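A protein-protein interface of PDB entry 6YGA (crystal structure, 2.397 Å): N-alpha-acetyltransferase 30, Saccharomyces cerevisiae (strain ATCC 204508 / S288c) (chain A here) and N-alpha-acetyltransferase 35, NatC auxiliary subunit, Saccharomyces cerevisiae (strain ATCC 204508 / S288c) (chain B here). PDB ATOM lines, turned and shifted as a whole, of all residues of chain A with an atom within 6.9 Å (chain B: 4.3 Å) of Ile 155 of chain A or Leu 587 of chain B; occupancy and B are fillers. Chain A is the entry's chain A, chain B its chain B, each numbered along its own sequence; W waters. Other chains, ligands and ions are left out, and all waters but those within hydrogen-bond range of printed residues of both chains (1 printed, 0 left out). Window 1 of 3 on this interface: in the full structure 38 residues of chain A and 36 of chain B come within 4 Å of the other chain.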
ATOM      1  N   ARG A  76      20.437  -5.196  14.484  1.00  0.00           N
ATOM      2  CA  ARG A  76      20.158  -5.713  13.152  1.00  0.00           C
ATOM      3  C   ARG A  76      19.967  -7.222  13.182  1.00  0.00           C
ATOM      4  O   ARG A  76      20.661  -7.935  13.914  1.00  0.00           O
ATOM      5  CB  ARG A  76      21.279  -5.341  12.168  1.00  0.00           C
ATOM      6  CG  ARG A  76      21.313  -3.851  11.847  1.00  0.00           C
ATOM      7  CD  ARG A  76      22.499  -3.458  10.976  1.00  0.00           C
ATOM      8  NE  ARG A  76      22.431  -4.020   9.628  1.00  0.00           N
ATOM      9  CZ  ARG A  76      21.700  -3.515   8.637  1.00  0.00           C
ATOM     10  NH1 ARG A  76      20.956  -2.436   8.837  1.00  0.00           N
ATOM     11  NH2 ARG A  76      21.707  -4.093   7.444  1.00  0.00           N
ATOM     12  N   ARG A  78      20.390 -10.637  11.241  1.00  0.00           N
ATOM     13  CA  ARG A  78      21.246 -11.214  10.211  1.00  0.00           C
ATOM     14  C   ARG A  78      20.734 -12.604   9.849  1.00  0.00           C
ATOM     15  O   ARG A  78      20.780 -13.527  10.672  1.00  0.00           O
ATOM     16  CB  ARG A  78      22.698 -11.278  10.682  1.00  0.00           C
ATOM     17  CG  ARG A  78      23.582 -12.163   9.818  1.00  0.00           C
ATOM     18  CD  ARG A  78      25.053 -11.929  10.100  1.00  0.00           C
ATOM     19  NE  ARG A  78      25.485 -10.612   9.645  1.00  0.00           N
ATOM     20  CZ  ARG A  78      26.714 -10.133   9.805  1.00  0.00           C
ATOM     21  NH1 ARG A  78      27.638 -10.863  10.413  1.00  0.00           N
ATOM     22  NH2 ARG A  78      27.020  -8.924   9.356  1.00  0.00           N
ATOM     23  N   ASP A 113      17.670  -7.863   8.230  1.00  0.00           N
ATOM     24  CA  ASP A 113      18.309  -6.684   7.667  1.00  0.00           C
ATOM     25  C   ASP A 113      19.391  -7.032   6.659  1.00  0.00           C
ATOM     26  O   ASP A 113      19.755  -6.179   5.843  1.00  0.00           O
ATOM     27  CB  ASP A 113      18.908  -5.828   8.785  1.00  0.00           C
ATOM     28  CG  ASP A 113      17.856  -5.289   9.733  1.00  0.00           C
ATOM     29  OD1 ASP A 113      16.929  -4.600   9.261  1.00  0.00           O
ATOM     30  OD2 ASP A 113      17.948  -5.559  10.948  1.00  0.00           O
ATOM     31  N   GLU A 114      19.900  -8.261   6.691  1.00  0.00           N
ATOM     32  CA  GLU A 114      20.984  -8.669   5.810  1.00  0.00           C
ATOM     33  C   GLU A 114      21.055 -10.188   5.792  1.00  0.00           C
ATOM     34  O   GLU A 114      20.585 -10.864   6.711  1.00  0.00           O
ATOM     35  CB  GLU A 114      22.321  -8.071   6.258  1.00  0.00           C
ATOM     36  CG  GLU A 114      22.758  -8.536   7.635  1.00  0.00           C
ATOM     37  CD  GLU A 114      23.726  -7.578   8.298  1.00  0.00           C
ATOM     38  OE1 GLU A 114      23.718  -6.383   7.941  1.00  0.00           O
ATOM     39  OE2 GLU A 114      24.493  -8.022   9.179  1.00  0.00           O
ATOM     40  N   ILE A 115      21.651 -10.715   4.726  1.00  0.00           N
ATOM     41  CA  ILE A 115      21.882 -12.144   4.565  1.00  0.00           C
ATOM     42  C   ILE A 115      23.383 -12.364   4.462  1.00  0.00           C
ATOM     43  O   ILE A 115      24.065 -11.663   3.707  1.00  0.00           O
ATOM     44  CB  ILE A 115      21.163 -12.695   3.321  1.00  0.00           C
ATOM     45  CG1 ILE A 115      19.707 -12.234   3.307  1.00  0.00           C
ATOM     46  CG2 ILE A 115      21.225 -14.214   3.300  1.00  0.00           C
ATOM     47  CD1 ILE A 115      18.886 -12.793   4.447  1.00  0.00           C
ATOM     48  N   MET A 116      23.893 -13.334   5.214  1.00  0.00           N
ATOM     49  CA  MET A 116      25.325 -13.612   5.210  1.00  0.00           C
ATOM     50  C   MET A 116      25.611 -15.084   4.921  1.00  0.00           C
ATOM     51  O   MET A 116      24.890 -15.967   5.383  1.00  0.00           O
ATOM     52  CB  MET A 116      25.948 -13.205   6.549  1.00  0.00           C
ATOM     53  CG  MET A 116      27.470 -13.205   6.573  1.00  0.00           C
ATOM     54  SD  MET A 116      28.253 -14.945   6.984  1.00  0.00           S
ATOM     55  CE  MET A 116      28.075 -14.901   8.924  1.00  0.00           C
ATOM     56  N   LEU A 117      26.666 -15.335   4.149  1.00  0.00           N
ATOM     57  CA  LEU A 117      27.115 -16.689   3.871  1.00  0.00           C
ATOM     58  C   LEU A 117      28.620 -16.671   3.658  1.00  0.00           C
ATOM     59  O   LEU A 117      29.220 -15.623   3.406  1.00  0.00           O
ATOM     60  CB  LEU A 117      26.401 -17.287   2.648  1.00  0.00           C
ATOM     61  CG  LEU A 117      26.725 -16.671   1.280  1.00  0.00           C
ATOM     62  CD1 LEU A 117      27.764 -17.495   0.530  1.00  0.00           C
ATOM     63  CD2 LEU A 117      25.468 -16.498   0.439  1.00  0.00           C
ATOM     64  N   GLY A 134      23.100  -9.677  -5.863  1.00  0.00           N
ATOM     65  CA  GLY A 134      23.459  -8.447  -5.190  1.00  0.00           C
ATOM     66  C   GLY A 134      24.455  -8.615  -4.070  1.00  0.00           C
ATOM     67  O   GLY A 134      24.885  -7.609  -3.493  1.00  0.00           O
ATOM     68  N   PHE A 135      24.820  -9.850  -3.733  1.00  0.00           N
ATOM     69  CA  PHE A 135      25.841 -10.083  -2.725  1.00  0.00           C
ATOM     70  C   PHE A 135      27.157  -9.442  -3.148  1.00  0.00           C
ATOM     71  O   PHE A 135      27.498  -9.408  -4.335  1.00  0.00           O
ATOM     72  CB  PHE A 135      26.048 -11.584  -2.511  1.00  0.00           C
ATOM     73  CG  PHE A 135      25.013 -12.236  -1.635  1.00  0.00           C
ATOM     74  CD1 PHE A 135      23.817 -12.693  -2.169  1.00  0.00           C
ATOM     75  CD2 PHE A 135      25.250 -12.419  -0.281  1.00  0.00           C
ATOM     76  CE1 PHE A 135      22.870 -13.306  -1.366  1.00  0.00           C
ATOM     77  CE2 PHE A 135      24.305 -13.031   0.530  1.00  0.00           C
ATOM     78  CZ  PHE A 135      23.115 -13.476  -0.013  1.00  0.00           C
ATOM     79  N   ILE A 136      27.895  -8.928  -2.166  1.00  0.00           N
ATOM     80  CA  ILE A 136      29.253  -8.455  -2.381  1.00  0.00           C
ATOM     81  C   ILE A 136      30.151  -9.077  -1.323  1.00  0.00           C
ATOM     82  O   ILE A 136      29.706  -9.451  -0.234  1.00  0.00           O
ATOM     83  CB  ILE A 136      29.367  -6.914  -2.352  1.00  0.00           C
ATOM     84  CG1 ILE A 136      28.816  -6.351  -1.041  1.00  0.00           C
ATOM     85  CG2 ILE A 136      28.661  -6.302  -3.555  1.00  0.00           C
ATOM     86  CD1 ILE A 136      28.960  -4.846  -0.918  1.00  0.00           C
ATOM     87  N   ARG A 137      31.429  -9.194  -1.667  1.00  0.00           N
ATOM     88  CA  ARG A 137      32.422  -9.758  -0.765  1.00  0.00           C
ATOM     89  C   ARG A 137      32.844  -8.712   0.259  1.00  0.00           C
ATOM     90  O   ARG A 137      33.270  -7.610  -0.101  1.00  0.00           O
ATOM     91  CB  ARG A 137      33.627 -10.250  -1.562  1.00  0.00           C
ATOM     92  CG  ARG A 137      33.231 -11.041  -2.798  1.00  0.00           C
ATOM     93  CD  ARG A 137      34.398 -11.283  -3.732  1.00  0.00           C
ATOM     94  NE  ARG A 137      33.947 -11.871  -4.990  1.00  0.00           N
ATOM     95  CZ  ARG A 137      34.729 -12.089  -6.042  1.00  0.00           C
ATOM     96  NH1 ARG A 137      36.015 -11.769  -5.997  1.00  0.00           N
ATOM     97  NH2 ARG A 137      34.222 -12.627  -7.142  1.00  0.00           N
ATOM     98  N   MET A 138      32.726  -9.060   1.533  1.00  0.00           N
ATOM     99  CA  MET A 138      33.034  -8.127   2.606  1.00  0.00           C
ATOM    100  C   MET A 138      34.281  -8.529   3.380  1.00  0.00           C
ATOM    101  O   MET A 138      34.783  -7.760   4.199  1.00  0.00           O
ATOM    102  CB  MET A 138      31.845  -8.007   3.563  1.00  0.00           C
ATOM    103  CG  MET A 138      30.646  -7.301   2.953  1.00  0.00           C
ATOM    104  SD  MET A 138      31.110  -5.508   2.344  1.00  0.00           S
ATOM    105  CE  MET A 138      31.518  -4.694   4.069  1.00  0.00           C
ATOM    106  N   LYS A 153      33.491 -13.851   2.612  1.00  0.00           N
ATOM    107  CA  LYS A 153      32.286 -13.579   3.379  1.00  0.00           C
ATOM    108  C   LYS A 153      31.382 -12.701   2.525  1.00  0.00           C
ATOM    109  O   LYS A 153      31.745 -11.565   2.202  1.00  0.00           O
ATOM    110  CB  LYS A 153      32.628 -12.890   4.699  1.00  0.00           C
ATOM    111  CG  LYS A 153      31.453 -12.684   5.634  1.00  0.00           C
ATOM    112  CD  LYS A 153      31.905 -12.049   6.937  1.00  0.00           C
ATOM    113  CE  LYS A 153      30.858 -12.215   8.019  1.00  0.00           C
ATOM    114  NZ  LYS A 153      31.407 -11.877   9.360  1.00  0.00           N
ATOM    115  N   LEU A 154      30.224 -13.232   2.142  1.00  0.00           N
ATOM    116  CA  LEU A 154      29.286 -12.529   1.278  1.00  0.00           C
ATOM    117  C   LEU A 154      28.124 -11.997   2.103  1.00  0.00           C
ATOM    118  O   LEU A 154      27.600 -12.696   2.974  1.00  0.00           O
ATOM    119  CB  LEU A 154      28.754 -13.445   0.175  1.00  0.00           C
ATOM    120  CG  LEU A 154      29.804 -14.103  -0.719  1.00  0.00           C
ATOM    121  CD1 LEU A 154      29.158 -14.981  -1.783  1.00  0.00           C
ATOM    122  CD2 LEU A 154      30.676 -13.044  -1.356  1.00  0.00           C
ATOM    123  N   ILE A 155      27.725 -10.758   1.816  1.00  0.00           N
ATOM    124  CA  ILE A 155      26.637 -10.088   2.518  1.00  0.00           C
ATOM    125  C   ILE A 155      25.727  -9.414   1.500  1.00  0.00           C
ATOM    126  O   ILE A 155      26.203  -8.739   0.579  1.00  0.00           O
ATOM    127  CB  ILE A 155      27.162  -9.057   3.536  1.00  0.00           C
ATOM    128  CG1 ILE A 155      27.989  -9.751   4.617  1.00  0.00           C
ATOM    129  CG2 ILE A 155      26.009  -8.285   4.161  1.00  0.00           C
ATOM    130  CD1 ILE A 155      28.391  -8.840   5.740  1.00  0.00           C
ATOM    131  N   LEU A 156      24.426  -9.608   1.663  1.00  0.00           N
ATOM    132  CA  LEU A 156      23.408  -8.956   0.845  1.00  0.00           C
ATOM    133  C   LEU A 156      22.572  -8.066   1.748  1.00  0.00           C
ATOM    134  O   LEU A 156      21.836  -8.579   2.615  1.00  0.00           O
ATOM    135  CB  LEU A 156      22.525  -9.984   0.140  1.00  0.00           C
ATOM    136  CG  LEU A 156      21.290  -9.458  -0.592  1.00  0.00           C
ATOM    137  CD1 LEU A 156      21.698  -8.696  -1.844  1.00  0.00           C
ATOM    138  CD2 LEU A 156      20.334 -10.597  -0.931  1.00  0.00           C
ATOM    139  N   PRO A 157      22.647  -6.745   1.595  1.00  0.00           N
ATOM    140  CA  PRO A 157      21.914  -5.845   2.494  1.00  0.00           C
ATOM    141  C   PRO A 157      20.465  -5.682   2.050  1.00  0.00           C
ATOM    142  O   PRO A 157      20.179  -5.431   0.875  1.00  0.00           O
ATOM    143  CB  PRO A 157      22.690  -4.530   2.378  1.00  0.00           C
ATOM    144  CG  PRO A 157      23.211  -4.553   0.987  1.00  0.00           C
ATOM    145  CD  PRO A 157      23.467  -6.004   0.622  1.00  0.00           C
ATOM    146  N   LEU B 583      21.914   0.648  -1.114  1.00  0.00           N
ATOM    147  CA  LEU B 583      22.272  -0.164   0.046  1.00  0.00           C
ATOM    148  C   LEU B 583      23.593  -0.887  -0.177  1.00  0.00           C
ATOM    149  O   LEU B 583      24.416  -0.992   0.740  1.00  0.00           O
ATOM    150  CB  LEU B 583      21.160  -1.168   0.351  1.00  0.00           C
ATOM    151  CG  LEU B 583      19.831  -0.592   0.844  1.00  0.00           C
ATOM    152  CD1 LEU B 583      18.790  -1.691   1.020  1.00  0.00           C
ATOM    153  CD2 LEU B 583      20.034   0.170   2.146  1.00  0.00           C
ATOM    154  N   ILE B 584      23.819  -1.386  -1.394  1.00  0.00           N
ATOM    155  CA  ILE B 584      25.056  -2.100  -1.688  1.00  0.00           C
ATOM    156  C   ILE B 584      26.242  -1.146  -1.666  1.00  0.00           C
ATOM    157  O   ILE B 584      27.323  -1.490  -1.171  1.00  0.00           O
ATOM    158  CB  ILE B 584      24.934  -2.837  -3.035  1.00  0.00           C
ATOM    159  CG1 ILE B 584      23.897  -3.955  -2.933  1.00  0.00           C
ATOM    160  CG2 ILE B 584      26.274  -3.405  -3.468  1.00  0.00           C
ATOM    161  CD1 ILE B 584      23.574  -4.597  -4.255  1.00  0.00           C
ATOM    162  N   HIS B 585      26.060   0.070  -2.188  1.00  0.00           N
ATOM    163  CA  HIS B 585      27.124   1.066  -2.131  1.00  0.00           C
ATOM    164  C   HIS B 585      27.468   1.435  -0.692  1.00  0.00           C
ATOM    165  O   HIS B 585      28.647   1.551  -0.342  1.00  0.00           O
ATOM    166  CB  HIS B 585      26.724   2.316  -2.911  1.00  0.00           C
ATOM    167  CG  HIS B 585      27.627   3.484  -2.669  1.00  0.00           C
ATOM    168  ND1 HIS B 585      28.768   3.709  -3.408  1.00  0.00           N
ATOM    169  CD2 HIS B 585      27.573   4.477  -1.749  1.00  0.00           C
ATOM    170  CE1 HIS B 585      29.370   4.798  -2.965  1.00  0.00           C
ATOM    171  NE2 HIS B 585      28.667   5.281  -1.957  1.00  0.00           N
ATOM    172  N   ASN B 586      26.454   1.633   0.154  1.00  0.00           N
ATOM    173  CA  ASN B 586      26.722   2.038   1.532  1.00  0.00           C
ATOM    174  C   ASN B 586      27.408   0.927   2.312  1.00  0.00           C
ATOM    175  O   ASN B 586      28.273   1.195   3.156  1.00  0.00           O
ATOM    176  CB  ASN B 586      25.426   2.450   2.229  1.00  0.00           C
ATOM    177  CG  ASN B 586      24.842   3.721   1.659  1.00  0.00           C
ATOM    178  OD1 ASN B 586      25.541   4.505   1.017  1.00  0.00           O
ATOM    179  ND2 ASN B 586      23.554   3.937   1.895  1.00  0.00           N
ATOM    180  N   LEU B 587      27.031  -0.325   2.051  1.00  0.00           N
ATOM    181  CA  LEU B 587      27.670  -1.450   2.725  1.00  0.00           C
ATOM    182  C   LEU B 587      29.155  -1.520   2.396  1.00  0.00           C
ATOM    183  O   LEU B 587      29.977  -1.833   3.266  1.00  0.00           O
ATOM    184  CB  LEU B 587      26.973  -2.751   2.332  1.00  0.00           C
ATOM    185  CG  LEU B 587      27.565  -4.037   2.908  1.00  0.00           C
ATOM    186  CD1 LEU B 587      27.362  -4.090   4.416  1.00  0.00           C
ATOM    187  CD2 LEU B 587      26.966  -5.266   2.235  1.00  0.00           C
ATOM    188  N   ARG B 588      29.519  -1.242   1.140  1.00  0.00           N
ATOM    189  CA  ARG B 588      30.921  -1.332   0.741  1.00  0.00           C
ATOM    190  C   ARG B 588      31.767  -0.299   1.472  1.00  0.00           C
ATOM    191  O   ARG B 588      32.908  -0.579   1.859  1.00  0.00           O
ATOM    192  CB  ARG B 588      31.043  -1.167  -0.778  1.00  0.00           C
ATOM    193  CG  ARG B 588      32.458  -0.895  -1.281  1.00  0.00           C
ATOM    194  CD  ARG B 588      33.390  -2.054  -0.988  1.00  0.00           C
ATOM    195  NE  ARG B 588      33.005  -3.259  -1.716  1.00  0.00           N
ATOM    196  CZ  ARG B 588      33.270  -4.493  -1.302  1.00  0.00           C
ATOM    197  NH1 ARG B 588      33.915  -4.683  -0.158  1.00  0.00           N
ATOM    198  NH2 ARG B 588      32.885  -5.535  -2.027  1.00  0.00           N
ATOM    199  N   PHE B 589      31.215   0.895   1.693  1.00  0.00           N
ATOM    200  CA  PHE B 589      31.932   1.996   2.316  1.00  0.00           C
ATOM    201  C   PHE B 589      31.609   2.149   3.798  1.00  0.00           C
ATOM    202  O   PHE B 589      31.983   3.159   4.405  1.00  0.00           O
ATOM    203  CB  PHE B 589      31.635   3.293   1.563  1.00  0.00           C
ATOM    204  CG  PHE B 589      32.219   3.328   0.177  1.00  0.00           C
ATOM    205  CD1 PHE B 589      31.511   2.827  -0.905  1.00  0.00           C
ATOM    206  CD2 PHE B 589      33.485   3.847  -0.037  1.00  0.00           C
ATOM    207  CE1 PHE B 589      32.053   2.855  -2.177  1.00  0.00           C
ATOM    208  CE2 PHE B 589      34.034   3.879  -1.305  1.00  0.00           C
ATOM    209  CZ  PHE B 589      33.317   3.382  -2.378  1.00  0.00           C
ATOM    210  N   LYS B 590      30.927   1.170   4.387  1.00  0.00           N
ATOM    211  CA  LYS B 590      30.679   1.176   5.828  1.00  0.00           C
ATOM    212  C   LYS B 590      31.933   1.390   6.676  1.00  0.00           C
ATOM    213  O   LYS B 590      31.838   2.125   7.673  1.00  0.00           O
ATOM    214  CB  LYS B 590      29.970  -0.130   6.218  1.00  0.00           C
ATOM    215  CG  LYS B 590      29.558  -0.243   7.681  1.00  0.00           C
ATOM    216  CD  LYS B 590      28.796  -1.545   7.906  1.00  0.00           C
ATOM    217  CE  LYS B 590      28.246  -1.652   9.316  1.00  0.00           C
ATOM    218  NZ  LYS B 590      29.319  -1.786  10.341  1.00  0.00           N
HETATM  219  O   HOH W   1      32.536  -7.980  -3.902  1.00  0.00           O
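The backbone carbonyl oxygen of Arg 137 of chain A sits at hydrogen-bond distance from the guanidinium group of Arg 588 of chain B.
The backbone carbonyl oxygen (O) of Ile 136 of chain A sits at hydrogen-bond distance from the backbone NH (N) of Ile 155 of chain A (3.1 Å). The backbone NH (N) of Met 138 of chain A is in hydrogen-bond range of the backbone carbonyl oxygen (O) of Lys 153 of chain A (2.8 Å).
Ile 584 of chain B touches Gly 134 of chain A (CD1 to O, 3.4 Å). Ile 584 of chain B touches Ile 136 of chain A (O to CD1, 3.7 Å). CD2 of Leu 587 of chain B touches CD1 of Ile 136 of chain A (3.8 Å). Arg 588 of chain B touches Ile 136 of chain A (NH2 to CB, 3.8 Å). Met 138 of chain A touches Leu 587 of chain B. Met 138 of chain A touches Arg 588 of chain B. CG2 of Ile 155 of chain A touches CD2 of Leu 587 of chain B (3.7 Å). Leu 583 of chain B touches Pro 157 of chain A. CD of Pro 157 of chain A touches CD2 of Leu 587 of chain B, at 3.9 Å.
Of the printed residues of chain B, Gly 134 of chain A touches Ile 584. Of the printed residues of chain B, Ile 136 of chain A touches Ile 584, Leu 587 and Arg 588. Printed residues of chain B within 4 Å of Ile 155 of chain A: Leu 587 (3.7 Å). Printed residues of chain B within 4 Å of Pro 157 of chain A: Leu 583 (3.8 Å) and Leu 587 (3.9 Å). Of the printed residues of chain A, Leu 583 of chain B touches Pro 157. Printed residues of chain A within 4 Å of Arg 588 of chain B: Ile 136 (3.8 Å), Arg 137 (2.9 Å) and Met 138 (3.8 Å). The nearest printed residue of chain B that does not touch Arg 137 of chain A is Leu 587 of chain B (7.1 Å).
Of the 17 printed residues of chain A, 6 touch a printed residue of chain B. Printed residues of chain A that touch a printed residue of chain B: Gly 134, Ile 136, Arg 137, Met 138, Ile 155 and Pro 157. Hydrophobic or aromatic side chains of chain A that line the printed part of chain B: Ile 136, Met 138, Ile 155 and Pro 157. Printed residues of chain B that touch a printed residue of chain A: Leu 583, Ile 584, Leu 587 and Arg 588. Hydrophobic or aromatic side chains of chain B that line the printed part of chain A: Leu 583, Ile 584 and Leu 587. Among the printed residues, no Asp or Glu carboxylate lies within 4 Å of a Lys or Arg side-chain nitrogen of the other chain.
Water W1 lies within hydrogen-bond range of N of Arg 137 of chain A (2.8 Å) and NH2 of Arg 588 of chain B (3.1 Å).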
